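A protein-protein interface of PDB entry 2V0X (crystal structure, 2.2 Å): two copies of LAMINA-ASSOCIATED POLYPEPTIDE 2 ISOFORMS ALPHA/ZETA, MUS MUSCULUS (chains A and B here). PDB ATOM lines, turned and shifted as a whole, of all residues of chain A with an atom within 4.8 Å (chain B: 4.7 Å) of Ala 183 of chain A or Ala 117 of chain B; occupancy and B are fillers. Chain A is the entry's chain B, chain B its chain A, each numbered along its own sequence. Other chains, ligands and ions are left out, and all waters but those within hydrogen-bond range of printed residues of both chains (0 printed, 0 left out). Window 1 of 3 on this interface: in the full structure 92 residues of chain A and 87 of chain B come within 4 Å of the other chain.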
ATOM      1  N   SER A 113      24.580 -20.991  -6.430  1.00  0.00           N
ATOM      2  CA  SER A 113      23.733 -22.169  -6.266  1.00  0.00           C
ATOM      3  C   SER A 113      22.731 -21.897  -5.136  1.00  0.00           C
ATOM      4  O   SER A 113      21.544 -22.174  -5.262  1.00  0.00           O
ATOM      5  CB  SER A 113      24.566 -23.403  -5.911  1.00  0.00           C
ATOM      6  OG  SER A 113      25.373 -23.809  -7.012  1.00  0.00           O
ATOM      7  N   ALA A 116      20.124 -19.180  -6.309  1.00  0.00           N
ATOM      8  CA  ALA A 116      19.164 -19.706  -7.279  1.00  0.00           C
ATOM      9  C   ALA A 116      18.118 -20.567  -6.562  1.00  0.00           C
ATOM     10  O   ALA A 116      16.917 -20.456  -6.837  1.00  0.00           O
ATOM     11  CB  ALA A 116      19.886 -20.526  -8.371  1.00  0.00           C
ATOM     12  N   MET A 179      15.063 -21.023 -12.501  1.00  0.00           N
ATOM     13  CA  MET A 179      15.933 -20.944 -11.332  1.00  0.00           C
ATOM     14  C   MET A 179      16.746 -22.229 -11.145  1.00  0.00           C
ATOM     15  O   MET A 179      17.939 -22.174 -10.806  1.00  0.00           O
ATOM     16  CB  MET A 179      15.132 -20.623 -10.064  1.00  0.00           C
ATOM     17  CG  MET A 179      14.515 -19.208 -10.022  1.00  0.00           C
ATOM     18  SD  MET A 179      15.751 -17.773 -10.577  1.00  0.00           S
ATOM     19  CE  MET A 179      17.262 -18.255  -9.559  1.00  0.00           C
ATOM     20  N   SER A 180      16.109 -23.380 -11.378  1.00  0.00           N
ATOM     21  CA  SER A 180      16.775 -24.679 -11.262  1.00  0.00           C
ATOM     22  C   SER A 180      17.884 -24.819 -12.311  1.00  0.00           C
ATOM     23  O   SER A 180      18.950 -25.350 -12.020  1.00  0.00           O
ATOM     24  CB  SER A 180      15.770 -25.832 -11.436  1.00  0.00           C
ATOM     25  OG  SER A 180      14.848 -25.888 -10.356  1.00  0.00           O
ATOM     26  N   ALA A 181      17.621 -24.334 -13.520  1.00  0.00           N
ATOM     27  CA  ALA A 181      18.591 -24.408 -14.604  1.00  0.00           C
ATOM     28  C   ALA A 181      19.815 -23.562 -14.264  1.00  0.00           C
ATOM     29  O   ALA A 181      20.944 -23.988 -14.502  1.00  0.00           O
ATOM     30  CB  ALA A 181      17.972 -23.956 -15.935  1.00  0.00           C
ATOM     31  N   CYS A 182      19.589 -22.417 -13.629  1.00  0.00           N
ATOM     32  CA  CYS A 182      20.670 -21.514 -13.233  1.00  0.00           C
ATOM     33  C   CYS A 182      21.536 -22.187 -12.177  1.00  0.00           C
ATOM     34  O   CYS A 182      22.767 -22.123 -12.238  1.00  0.00           O
ATOM     35  CB  CYS A 182      20.100 -20.199 -12.679  1.00  0.00           C
ATOM     36  SG  CYS A 182      19.407 -19.062 -13.935  1.00  0.00           S
ATOM     37  N   ALA A 183      20.885 -22.833 -11.209  1.00  0.00           N
ATOM     38  CA  ALA A 183      21.584 -23.528 -10.134  1.00  0.00           C
ATOM     39  C   ALA A 183      22.468 -24.625 -10.722  1.00  0.00           C
ATOM     40  O   ALA A 183      23.616 -24.785 -10.329  1.00  0.00           O
ATOM     41  CB  ALA A 183      20.588 -24.130  -9.150  1.00  0.00           C
ATOM     42  N   MET A 184      21.896 -25.399 -11.635  1.00  0.00           N
ATOM     43  CA  MET A 184      22.607 -26.471 -12.314  1.00  0.00           C
ATOM     44  C   MET A 184      23.782 -25.892 -13.112  1.00  0.00           C
ATOM     45  O   MET A 184      24.856 -26.477 -13.145  1.00  0.00           O
ATOM     46  CB  MET A 184      21.639 -27.227 -13.234  1.00  0.00           C
ATOM     47  CG  MET A 184      20.652 -28.131 -12.476  1.00  0.00           C
ATOM     48  SD  MET A 184      18.998 -28.427 -13.456  1.00  0.00           S
ATOM     49  CE  MET A 184      19.486 -30.003 -14.447  1.00  0.00           C
ATOM     50  N   GLY A 185      23.563 -24.759 -13.773  1.00  0.00           N
ATOM     51  CA  GLY A 185      24.635 -24.113 -14.510  1.00  0.00           C
ATOM     52  C   GLY A 185      25.765 -23.690 -13.564  1.00  0.00           C
ATOM     53  O   GLY A 185      26.927 -23.920 -13.843  1.00  0.00           O
ATOM     54  N   SER A 186      25.416 -23.119 -12.415  1.00  0.00           N
ATOM     55  CA  SER A 186      26.407 -22.667 -11.441  1.00  0.00           C
ATOM     56  C   SER A 186      27.178 -23.837 -10.851  1.00  0.00           C
ATOM     57  O   SER A 186      28.399 -23.764 -10.683  1.00  0.00           O
ATOM     58  CB  SER A 186      25.737 -21.849 -10.344  1.00  0.00           C
ATOM     59  OG  SER A 186      25.152 -20.691 -10.903  1.00  0.00           O
ATOM     60  N   SER A 187      26.469 -24.921 -10.563  1.00  0.00           N
ATOM     61  CA  SER A 187      27.101 -26.114 -10.026  1.00  0.00           C
ATOM     62  C   SER A 187      28.149 -26.615 -11.040  1.00  0.00           C
ATOM     63  O   SER A 187      29.291 -26.900 -10.684  1.00  0.00           O
ATOM     64  CB  SER A 187      26.048 -27.198  -9.781  1.00  0.00           C
ATOM     65  OG  SER A 187      26.651 -28.482  -9.688  1.00  0.00           O
ATOM     66  N   SER B 113      24.184 -30.124  -5.118  1.00  0.00           N
ATOM     67  CA  SER B 113      23.494 -28.888  -5.473  1.00  0.00           C
ATOM     68  C   SER B 113      22.811 -29.109  -6.826  1.00  0.00           C
ATOM     69  O   SER B 113      21.665 -28.704  -7.043  1.00  0.00           O
ATOM     70  CB  SER B 113      24.485 -27.714  -5.612  1.00  0.00           C
ATOM     71  OG  SER B 113      25.222 -27.492  -4.424  1.00  0.00           O
ATOM     72  N   TYR B 114      23.552 -29.710  -7.749  1.00  0.00           N
ATOM     73  CA  TYR B 114      23.017 -29.989  -9.082  1.00  0.00           C
ATOM     74  C   TYR B 114      21.843 -30.977  -8.968  1.00  0.00           C
ATOM     75  O   TYR B 114      20.804 -30.782  -9.570  1.00  0.00           O
ATOM     76  CB  TYR B 114      24.107 -30.605  -9.989  1.00  0.00           C
ATOM     77  CG  TYR B 114      23.716 -30.734 -11.459  1.00  0.00           C
ATOM     78  CD1 TYR B 114      24.207 -29.838 -12.408  1.00  0.00           C
ATOM     79  CD2 TYR B 114      22.829 -31.732 -11.895  1.00  0.00           C
ATOM     80  CE1 TYR B 114      23.825 -29.923 -13.755  1.00  0.00           C
ATOM     81  CE2 TYR B 114      22.434 -31.824 -13.252  1.00  0.00           C
ATOM     82  CZ  TYR B 114      22.935 -30.917 -14.164  1.00  0.00           C
ATOM     83  OH  TYR B 114      22.549 -30.961 -15.488  1.00  0.00           O
ATOM     84  N   GLU B 115      22.016 -32.020  -8.168  1.00  0.00           N
ATOM     85  CA  GLU B 115      20.992 -33.052  -8.034  1.00  0.00           C
ATOM     86  C   GLU B 115      19.706 -32.504  -7.394  1.00  0.00           C
ATOM     87  O   GLU B 115      18.610 -32.778  -7.875  1.00  0.00           O
ATOM     88  CB  GLU B 115      21.549 -34.227  -7.238  1.00  0.00           C
ATOM     89  CG  GLU B 115      20.746 -35.493  -7.316  1.00  0.00           C
ATOM     90  CD  GLU B 115      21.277 -36.575  -6.389  1.00  0.00           C
ATOM     91  OE1 GLU B 115      22.519 -36.744  -6.300  1.00  0.00           O
ATOM     92  OE2 GLU B 115      20.444 -37.254  -5.748  1.00  0.00           O
ATOM     93  N   ALA B 116      19.859 -31.656  -6.376  1.00  0.00           N
ATOM     94  CA  ALA B 116      18.706 -31.067  -5.691  1.00  0.00           C
ATOM     95  C   ALA B 116      17.947 -30.140  -6.649  1.00  0.00           C
ATOM     96  O   ALA B 116      16.702 -30.145  -6.694  1.00  0.00           O
ATOM     97  CB  ALA B 116      19.155 -30.315  -4.438  1.00  0.00           C
ATOM     98  N   ALA B 117      18.700 -29.383  -7.448  1.00  0.00           N
ATOM     99  CA  ALA B 117      18.104 -28.473  -8.424  1.00  0.00           C
ATOM    100  C   ALA B 117      17.419 -29.230  -9.573  1.00  0.00           C
ATOM    101  O   ALA B 117      16.406 -28.771 -10.110  1.00  0.00           O
ATOM    102  CB  ALA B 117      19.179 -27.530  -8.983  1.00  0.00           C
ATOM    103  N   ALA B 118      18.017 -30.347  -9.993  1.00  0.00           N
ATOM    104  CA  ALA B 118      17.460 -31.182 -11.072  1.00  0.00           C
ATOM    105  C   ALA B 118      16.116 -31.744 -10.610  1.00  0.00           C
ATOM    106  O   ALA B 118      15.142 -31.746 -11.347  1.00  0.00           O
ATOM    107  CB  ALA B 118      18.431 -32.339 -11.425  1.00  0.00           C
ATOM    108  N   SER B 119      16.074 -32.186  -9.365  1.00  0.00           N
ATOM    109  CA  SER B 119      14.856 -32.728  -8.780  1.00  0.00           C
ATOM    110  C   SER B 119      13.768 -31.663  -8.718  1.00  0.00           C
ATOM    111  O   SER B 119      12.619 -31.922  -9.079  1.00  0.00           O
ATOM    112  CB  SER B 119      15.162 -33.265  -7.392  1.00  0.00           C
ATOM    113  OG  SER B 119      16.036 -34.373  -7.500  1.00  0.00           O
ATOM    114  N   ALA B 120      14.139 -30.452  -8.296  1.00  0.00           N
ATOM    115  CA  ALA B 120      13.201 -29.326  -8.226  1.00  0.00           C
ATOM    116  C   ALA B 120      12.670 -29.046  -9.634  1.00  0.00           C
ATOM    117  O   ALA B 120      11.496 -28.709  -9.830  1.00  0.00           O
ATOM    118  CB  ALA B 120      13.916 -28.074  -7.680  1.00  0.00           C
ATOM    119  N   LEU B 121      13.537 -29.179 -10.627  1.00  0.00           N
ATOM    120  CA  LEU B 121      13.119 -28.944 -11.994  1.00  0.00           C
ATOM    121  C   LEU B 121      12.137 -30.022 -12.460  1.00  0.00           C
ATOM    122  O   LEU B 121      11.156 -29.726 -13.136  1.00  0.00           O
ATOM    123  CB  LEU B 121      14.339 -28.869 -12.892  1.00  0.00           C
ATOM    124  CG  LEU B 121      14.343 -28.902 -14.422  1.00  0.00           C
ATOM    125  CD1 LEU B 121      13.068 -28.466 -15.061  1.00  0.00           C
ATOM    126  CD2 LEU B 121      15.526 -28.052 -14.900  1.00  0.00           C
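O of Ala 117 of chain B lies within hydrogen-bond range of OG of Ser 180 of chain A (3.3 Å).
Among the printed residues, merely in contact across the chains: Ser 187 of chain A with Tyr 114 of chain B (3.3 Å), Met 184 of chain A with Tyr 114 of chain B (3.4 Å), Ser 180 of chain A with Leu 121 of chain B (3.6 Å), Ser 180 of chain A with Ala 120 of chain B (3.6 Å), Ala 183 of chain A with Ala 117 of chain B (3.7 Å), Met 184 of chain A with Leu 121 of chain B (3.8 Å), Met 184 of chain A with Ala 117 of chain B (3.8 Å) and Met 184 of chain A with Ala 118 of chain B (3.95 Å).
Ala 183 of chain A touches one residue of chain B. Of the printed residues of chain B, Ser 187 of chain A touches Tyr 114. Printed residues of chain A within 4 Å of Tyr 114 of chain B: Met 184 and Ser 187. Ala 117 of chain B touches three residues of chain A.
Hydrophobic or aromatic side chains of chain A within 4 Å of the printed part of chain B: Ala 183 and Met 184. Printed residues of chain B that touch a printed residue of chain A: Tyr 114, Ala 117, Ala 118, Ala 120 and Leu 121. Among the printed residues, no Asp or Glu carboxylate lies within 4 Å of a Lys or Arg side-chain nitrogen of the other chain.
2 positions are printed for both chains. Of the 9 pairs that touch across the chains among the printed residues, none has its exchanged pair printed and touching as well.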
